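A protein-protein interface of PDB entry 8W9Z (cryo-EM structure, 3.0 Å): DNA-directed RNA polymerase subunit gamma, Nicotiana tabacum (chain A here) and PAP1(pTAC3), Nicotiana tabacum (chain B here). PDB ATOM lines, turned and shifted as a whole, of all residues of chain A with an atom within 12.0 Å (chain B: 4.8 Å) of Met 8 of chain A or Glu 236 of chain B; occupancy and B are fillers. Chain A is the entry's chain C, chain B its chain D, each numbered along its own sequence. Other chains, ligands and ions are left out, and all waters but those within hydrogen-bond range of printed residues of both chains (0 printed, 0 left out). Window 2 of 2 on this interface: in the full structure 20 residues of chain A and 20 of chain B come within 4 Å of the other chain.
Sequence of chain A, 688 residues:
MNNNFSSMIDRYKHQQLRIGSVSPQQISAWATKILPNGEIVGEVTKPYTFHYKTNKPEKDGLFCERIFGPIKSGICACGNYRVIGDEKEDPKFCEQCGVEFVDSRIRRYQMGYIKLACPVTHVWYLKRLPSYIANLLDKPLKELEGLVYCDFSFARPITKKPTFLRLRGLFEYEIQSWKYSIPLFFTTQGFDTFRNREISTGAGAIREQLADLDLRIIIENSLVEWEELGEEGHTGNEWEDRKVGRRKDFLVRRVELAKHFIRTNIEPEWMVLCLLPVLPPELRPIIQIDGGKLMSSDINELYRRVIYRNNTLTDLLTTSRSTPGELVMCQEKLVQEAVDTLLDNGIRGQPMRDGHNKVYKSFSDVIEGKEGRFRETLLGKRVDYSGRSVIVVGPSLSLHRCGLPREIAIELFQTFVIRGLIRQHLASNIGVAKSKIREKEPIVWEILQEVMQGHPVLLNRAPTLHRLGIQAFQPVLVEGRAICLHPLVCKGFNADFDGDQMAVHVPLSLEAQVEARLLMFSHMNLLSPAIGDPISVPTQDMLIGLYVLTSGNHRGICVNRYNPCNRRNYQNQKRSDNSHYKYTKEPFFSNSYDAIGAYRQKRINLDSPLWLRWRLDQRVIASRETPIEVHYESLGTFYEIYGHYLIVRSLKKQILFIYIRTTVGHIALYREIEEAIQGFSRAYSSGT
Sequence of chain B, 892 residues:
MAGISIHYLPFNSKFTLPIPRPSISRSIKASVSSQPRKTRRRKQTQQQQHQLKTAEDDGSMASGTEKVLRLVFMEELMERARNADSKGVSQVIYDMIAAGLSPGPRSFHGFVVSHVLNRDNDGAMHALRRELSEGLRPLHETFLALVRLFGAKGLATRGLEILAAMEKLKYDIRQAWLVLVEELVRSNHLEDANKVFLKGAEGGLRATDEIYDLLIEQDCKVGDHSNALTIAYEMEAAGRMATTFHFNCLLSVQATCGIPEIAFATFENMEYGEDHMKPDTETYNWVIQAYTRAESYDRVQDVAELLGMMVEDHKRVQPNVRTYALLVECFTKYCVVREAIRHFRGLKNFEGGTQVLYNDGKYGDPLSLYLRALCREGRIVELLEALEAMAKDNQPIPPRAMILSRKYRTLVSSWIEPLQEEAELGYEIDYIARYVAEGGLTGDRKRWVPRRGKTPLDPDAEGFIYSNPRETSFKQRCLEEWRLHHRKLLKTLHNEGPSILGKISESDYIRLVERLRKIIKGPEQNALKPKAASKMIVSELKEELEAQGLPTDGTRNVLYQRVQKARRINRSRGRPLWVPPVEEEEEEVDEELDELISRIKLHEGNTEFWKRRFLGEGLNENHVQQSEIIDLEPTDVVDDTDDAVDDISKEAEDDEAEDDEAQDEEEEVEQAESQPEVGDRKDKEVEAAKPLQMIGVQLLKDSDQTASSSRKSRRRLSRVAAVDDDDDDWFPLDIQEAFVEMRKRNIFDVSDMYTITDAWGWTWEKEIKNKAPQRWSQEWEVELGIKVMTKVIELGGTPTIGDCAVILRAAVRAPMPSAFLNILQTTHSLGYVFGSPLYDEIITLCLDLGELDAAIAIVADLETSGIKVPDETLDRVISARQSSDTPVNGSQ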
ATOM      1  N   MET A   8       9.529  24.866  24.814  1.00  0.00           N
ATOM      2  CA  MET A   8      10.119  24.743  26.142  1.00  0.00           C
ATOM      3  C   MET A   8      11.591  24.355  26.053  1.00  0.00           C
ATOM      4  O   MET A   8      11.923  23.216  25.725  1.00  0.00           O
ATOM      5  CB  MET A   8       9.354  23.715  26.976  1.00  0.00           C
ATOM      6  N   ILE A   9      12.469  25.309  26.346  1.00  0.00           N
ATOM      7  CA  ILE A   9      13.905  25.060  26.310  1.00  0.00           C
ATOM      8  C   ILE A   9      14.314  24.327  27.579  1.00  0.00           C
ATOM      9  O   ILE A   9      13.934  24.719  28.689  1.00  0.00           O
ATOM     10  CB  ILE A   9      14.681  26.377  26.156  1.00  0.00           C
ATOM     11  CG1 ILE A   9      14.228  27.122  24.902  1.00  0.00           C
ATOM     12  CG2 ILE A   9      16.175  26.110  26.094  1.00  0.00           C
ATOM     13  CD1 ILE A   9      14.926  28.444  24.696  1.00  0.00           C
ATOM     14  N   ASP A  10      15.087  23.257  27.419  1.00  0.00           N
ATOM     15  CA  ASP A  10      15.567  22.501  28.564  1.00  0.00           C
ATOM     16  C   ASP A  10      16.665  23.277  29.289  1.00  0.00           C
ATOM     17  O   ASP A  10      17.172  24.296  28.809  1.00  0.00           O
ATOM     18  CB  ASP A  10      16.081  21.132  28.124  1.00  0.00           C
ATOM     19  CG  ASP A  10      15.018  20.307  27.427  1.00  0.00           C
ATOM     20  OD1 ASP A  10      13.824  20.473  27.755  1.00  0.00           O
ATOM     21  OD2 ASP A  10      15.375  19.492  26.550  1.00  0.00           O
ATOM     22  N   ARG A  11      17.036  22.778  30.469  1.00  0.00           N
ATOM     23  CA  ARG A  11      18.073  23.432  31.258  1.00  0.00           C
ATOM     24  C   ARG A  11      19.461  23.244  30.659  1.00  0.00           C
ATOM     25  O   ARG A  11      20.353  24.052  30.940  1.00  0.00           O
ATOM     26  CB  ARG A  11      18.046  22.913  32.696  1.00  0.00           C
ATOM     27  CG  ARG A  11      16.760  23.237  33.438  1.00  0.00           C
ATOM     28  CD  ARG A  11      16.493  24.734  33.442  1.00  0.00           C
ATOM     29  NE  ARG A  11      15.252  25.069  34.132  1.00  0.00           N
ATOM     30  CZ  ARG A  11      14.783  26.305  34.267  1.00  0.00           C
ATOM     31  NH1 ARG A  11      13.643  26.518  34.911  1.00  0.00           N
ATOM     32  NH2 ARG A  11      15.453  27.329  33.758  1.00  0.00           N
ATOM     33  N   TYR A  12      19.657  22.203  29.849  1.00  0.00           N
ATOM     34  CA  TYR A  12      20.911  21.964  29.132  1.00  0.00           C
ATOM     35  C   TYR A  12      22.095  21.842  30.096  1.00  0.00           C
ATOM     36  O   TYR A  12      23.037  22.636  30.073  1.00  0.00           O
ATOM     37  CB  TYR A  12      21.163  23.057  28.089  1.00  0.00           C
ATOM     38  CG  TYR A  12      20.173  23.070  26.947  1.00  0.00           C
ATOM     39  CD1 TYR A  12      19.448  21.934  26.615  1.00  0.00           C
ATOM     40  CD2 TYR A  12      19.964  24.220  26.197  1.00  0.00           C
ATOM     41  CE1 TYR A  12      18.544  21.944  25.573  1.00  0.00           C
ATOM     42  CE2 TYR A  12      19.063  24.239  25.154  1.00  0.00           C
ATOM     43  CZ  TYR A  12      18.355  23.099  24.846  1.00  0.00           C
ATOM     44  OH  TYR A  12      17.454  23.115  23.805  1.00  0.00           O
ATOM     45  N   LYS A  13      22.029  20.827  30.951  1.00  0.00           N
ATOM     46  CA  LYS A  13      23.149  20.483  31.816  1.00  0.00           C
ATOM     47  C   LYS A  13      24.082  19.531  31.079  1.00  0.00           C
ATOM     48  O   LYS A  13      23.636  18.583  30.427  1.00  0.00           O
ATOM     49  CB  LYS A  13      22.661  19.858  33.125  1.00  0.00           C
ATOM     50  N   ALA B 232      16.000  34.215  26.266  1.00  0.00           N
ATOM     51  CA  ALA B 232      15.094  33.163  25.816  1.00  0.00           C
ATOM     52  C   ALA B 232      14.364  32.518  26.989  1.00  0.00           C
ATOM     53  O   ALA B 232      13.160  32.236  26.903  1.00  0.00           O
ATOM     54  CB  ALA B 232      15.863  32.111  25.018  1.00  0.00           C
ATOM     55  N   TYR B 233      15.075  32.273  28.092  1.00  0.00           N
ATOM     56  CA  TYR B 233      14.428  31.737  29.284  1.00  0.00           C
ATOM     57  C   TYR B 233      13.383  32.705  29.824  1.00  0.00           C
ATOM     58  O   TYR B 233      12.281  32.291  30.205  1.00  0.00           O
ATOM     59  CB  TYR B 233      15.470  31.425  30.357  1.00  0.00           C
ATOM     60  CG  TYR B 233      16.269  30.167  30.101  1.00  0.00           C
ATOM     61  CD1 TYR B 233      15.770  29.158  29.291  1.00  0.00           C
ATOM     62  CD2 TYR B 233      17.519  29.988  30.676  1.00  0.00           C
ATOM     63  CE1 TYR B 233      16.495  28.006  29.060  1.00  0.00           C
ATOM     64  CE2 TYR B 233      18.251  28.840  30.449  1.00  0.00           C
ATOM     65  CZ  TYR B 233      17.734  27.853  29.641  1.00  0.00           C
ATOM     66  OH  TYR B 233      18.461  26.708  29.411  1.00  0.00           O
ATOM     67  N   GLU B 234      13.707  34.000  29.860  1.00  0.00           N
ATOM     68  CA  GLU B 234      12.739  34.987  30.332  1.00  0.00           C
ATOM     69  C   GLU B 234      11.534  35.070  29.403  1.00  0.00           C
ATOM     70  O   GLU B 234      10.403  35.271  29.859  1.00  0.00           O
ATOM     71  CB  GLU B 234      13.406  36.356  30.473  1.00  0.00           C
ATOM     72  CG  GLU B 234      14.468  36.424  31.558  1.00  0.00           C
ATOM     73  CD  GLU B 234      13.891  36.288  32.956  1.00  0.00           C
ATOM     74  OE1 GLU B 234      12.689  36.574  33.137  1.00  0.00           O
ATOM     75  OE2 GLU B 234      14.642  35.895  33.873  1.00  0.00           O
ATOM     76  N   MET B 235      11.757  34.912  28.097  1.00  0.00           N
ATOM     77  CA  MET B 235      10.656  34.914  27.141  1.00  0.00           C
ATOM     78  C   MET B 235       9.731  33.729  27.373  1.00  0.00           C
ATOM     79  O   MET B 235       8.504  33.880  27.411  1.00  0.00           O
ATOM     80  CB  MET B 235      11.207  34.890  25.716  1.00  0.00           C
ATOM     81  CG  MET B 235      10.145  34.778  24.641  1.00  0.00           C
ATOM     82  SD  MET B 235      10.802  34.134  23.092  1.00  0.00           S
ATOM     83  CE  MET B 235      12.156  35.265  22.806  1.00  0.00           C
ATOM     84  N   GLU B 236      10.304  32.533  27.529  1.00  0.00           N
ATOM     85  CA  GLU B 236       9.479  31.355  27.768  1.00  0.00           C
ATOM     86  C   GLU B 236       8.789  31.414  29.125  1.00  0.00           C
ATOM     87  O   GLU B 236       7.709  30.836  29.293  1.00  0.00           O
ATOM     88  CB  GLU B 236      10.316  30.084  27.647  1.00  0.00           C
ATOM     89  CG  GLU B 236      10.648  29.708  26.215  1.00  0.00           C
ATOM     90  CD  GLU B 236      11.165  28.290  26.090  1.00  0.00           C
ATOM     91  OE1 GLU B 236      11.652  27.741  27.101  1.00  0.00           O
ATOM     92  OE2 GLU B 236      11.079  27.723  24.981  1.00  0.00           O
ATOM     93  N   ALA B 237       9.388  32.101  30.099  1.00  0.00           N
ATOM     94  CA  ALA B 237       8.734  32.254  31.393  1.00  0.00           C
ATOM     95  C   ALA B 237       7.604  33.273  31.335  1.00  0.00           C
ATOM     96  O   ALA B 237       6.604  33.129  32.046  1.00  0.00           O
ATOM     97  CB  ALA B 237       9.757  32.655  32.457  1.00  0.00           C
ATOM     98  N   ALA B 238       7.742  34.306  30.499  1.00  0.00           N
ATOM     99  CA  ALA B 238       6.691  35.310  30.385  1.00  0.00           C
ATOM    100  C   ALA B 238       5.450  34.756  29.698  1.00  0.00           C
ATOM    101  O   ALA B 238       4.340  35.242  29.943  1.00  0.00           O
ATOM    102  CB  ALA B 238       7.212  36.534  29.632  1.00  0.00           C
ATOM    103  N   GLY B 239       5.609  33.749  28.844  1.00  0.00           N
ATOM    104  CA  GLY B 239       4.470  33.138  28.188  1.00  0.00           C
ATOM    105  C   GLY B 239       4.699  32.767  26.737  1.00  0.00           C
ATOM    106  O   GLY B 239       4.101  31.808  26.240  1.00  0.00           O
ATOM    107  N   ARG B 240       5.555  33.512  26.042  1.00  0.00           N
ATOM    108  CA  ARG B 240       5.829  33.240  24.637  1.00  0.00           C
ATOM    109  C   ARG B 240       6.872  32.136  24.524  1.00  0.00           C
ATOM    110  O   ARG B 240       7.991  32.277  25.030  1.00  0.00           O
ATOM    111  CB  ARG B 240       6.310  34.502  23.926  1.00  0.00           C
ATOM    112  CG  ARG B 240       6.517  34.312  22.434  1.00  0.00           C
ATOM    113  CD  ARG B 240       7.334  35.439  21.831  1.00  0.00           C
ATOM    114  NE  ARG B 240       7.502  35.270  20.391  1.00  0.00           N
ATOM    115  CZ  ARG B 240       8.327  35.995  19.644  1.00  0.00           C
ATOM    116  NH1 ARG B 240       9.072  36.941  20.201  1.00  0.00           N
ATOM    117  NH2 ARG B 240       8.414  35.772  18.340  1.00  0.00           N
ATOM    118  N   MET B 241       6.513  31.044  23.856  1.00  0.00           N
ATOM    119  CA  MET B 241       7.436  29.937  23.679  1.00  0.00           C
ATOM    120  C   MET B 241       8.348  30.188  22.481  1.00  0.00           C
ATOM    121  O   MET B 241       8.018  30.938  21.557  1.00  0.00           O
ATOM    122  CB  MET B 241       6.674  28.625  23.498  1.00  0.00           C
ATOM    123  CG  MET B 241       5.836  28.227  24.701  1.00  0.00           C
ATOM    124  SD  MET B 241       4.966  26.667  24.457  1.00  0.00           S
ATOM    125  CE  MET B 241       4.115  26.507  26.025  1.00  0.00           C
ATOM    126  N   ALA B 242       9.513  29.547  22.511  1.00  0.00           N
ATOM    127  CA  ALA B 242      10.514  29.764  21.476  1.00  0.00           C
ATOM    128  C   ALA B 242      10.109  29.086  20.173  1.00  0.00           C
ATOM    129  O   ALA B 242       9.513  28.005  20.173  1.00  0.00           O
ATOM    130  CB  ALA B 242      11.873  29.243  21.939  1.00  0.00           C
ATOM    131  N   ASN B 269      15.931  18.748  20.994  1.00  0.00           N
ATOM    132  CA  ASN B 269      14.843  19.527  21.573  1.00  0.00           C
ATOM    133  C   ASN B 269      13.913  20.067  20.495  1.00  0.00           C
ATOM    134  O   ASN B 269      12.701  20.171  20.715  1.00  0.00           O
ATOM    135  CB  ASN B 269      15.409  20.670  22.414  1.00  0.00           C
ATOM    136  CG  ASN B 269      14.342  21.406  23.191  1.00  0.00           C
ATOM    137  OD1 ASN B 269      13.831  22.433  22.746  1.00  0.00           O
ATOM    138  ND2 ASN B 269      13.997  20.886  24.362  1.00  0.00           N
ATOM    139  N   MET B 277       8.173  24.616  16.558  1.00  0.00           N
ATOM    140  CA  MET B 277       9.611  24.582  16.790  1.00  0.00           C
ATOM    141  C   MET B 277      10.303  23.476  15.999  1.00  0.00           C
ATOM    142  O   MET B 277      11.419  23.078  16.346  1.00  0.00           O
ATOM    143  CB  MET B 277       9.904  24.430  18.282  1.00  0.00           C
ATOM    144  CG  MET B 277       9.333  23.170  18.905  1.00  0.00           C
ATOM    145  SD  MET B 277       9.644  23.078  20.677  1.00  0.00           S
ATOM    146  CE  MET B 277      11.430  23.184  20.708  1.00  0.00           C
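Ile 9 of chain A touches Ala 232 of chain B (CD1 to CB, 3.8 Å). Tyr 233 of chain B touches Ile 9 of chain A (CE1 to CG2, 3.5 Å). Arg 11 of chain A touches Tyr 233 of chain B. Tyr 12 of chain A touches Asn 269 of chain B (OH to CB, 3.5 Å).
The backbone NH (N) of Met 8 of chain A is in hydrogen-bond range of the side-chain carboxylate (OE2) of Glu 236 of chain B (3.3 Å). O of Met 8 of chain A lies within hydrogen-bond range of ND2 of Asn 269 of chain B (3.4 Å). N of Ile 9 of chain A sits at hydrogen-bond distance from OE1 of Glu 236 of chain B (2.7 Å). O of Asp 10 of chain A is in hydrogen-bond range of OH of Tyr 233 of chain B, 2.8 Å away. The side-chain amide nitrogen (ND2) of Asn 269 of chain B lies within hydrogen-bond range of the side-chain carboxylate (OD2) of Asp 10 of chain A, at 2.9 Å.
Of the printed residues of chain B, Met 8 of chain A touches Glu 236 and Asn 269. Of the printed residues of chain A, Glu 236 of chain B touches Met 8 and Ile 9. Ala 232 of chain B touches just one residue of chain A: Ile 9 (3.8 Å). Tyr 233 of chain B touches just these residues of chain A: Ile 9, Asp 10 and Arg 11. No residue of chain A comes within 4 Å of Met 235 of chain B. No residue of chain A comes within 4 Å of Ala 237 of chain B. No residue of chain A comes within 4 Å of Gly 239 of chain B. No residue of chain A comes within 4 Å of Met 241 of chain B. Of chain A, only Met 8, Asp 10 and Tyr 12 come within 4 Å of Asn 269 of chain B. Of the printed residues of chain B, Ile 9 of chain A touches Ala 232, Tyr 233 and Glu 236. Of the printed residues of chain B, Asp 10 of chain A touches Tyr 233 (2.8 Å) and Asn 269 (2.9 Å). The nearest printed residue of chain B that does not touch Asp 10 of chain A is Glu 236 of chain B (5.7 Å).
Of the 13 printed residues of chain B, 4 touch a printed residue of chain A. Hydrophobic or aromatic side chains of chain B within 4 Å of the printed part of chain A: Ala 232 and Tyr 233. Of the 6 printed residues of chain A, 5 touch a printed residue of chain B. Printed residues of chain A that touch a printed residue of chain B: Met 8, Ile 9, Asp 10, Arg 11 and Tyr 12. Hydrophobic or aromatic side chains of chain A within 4 Å of the printed part of chain B: Ile 9 and Tyr 12. Among the printed residues, 9 pairs touch across the chains.
N of Ala 242 of chain B is in hydrogen-bond range of OE2 of Glu 236 of chain B.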
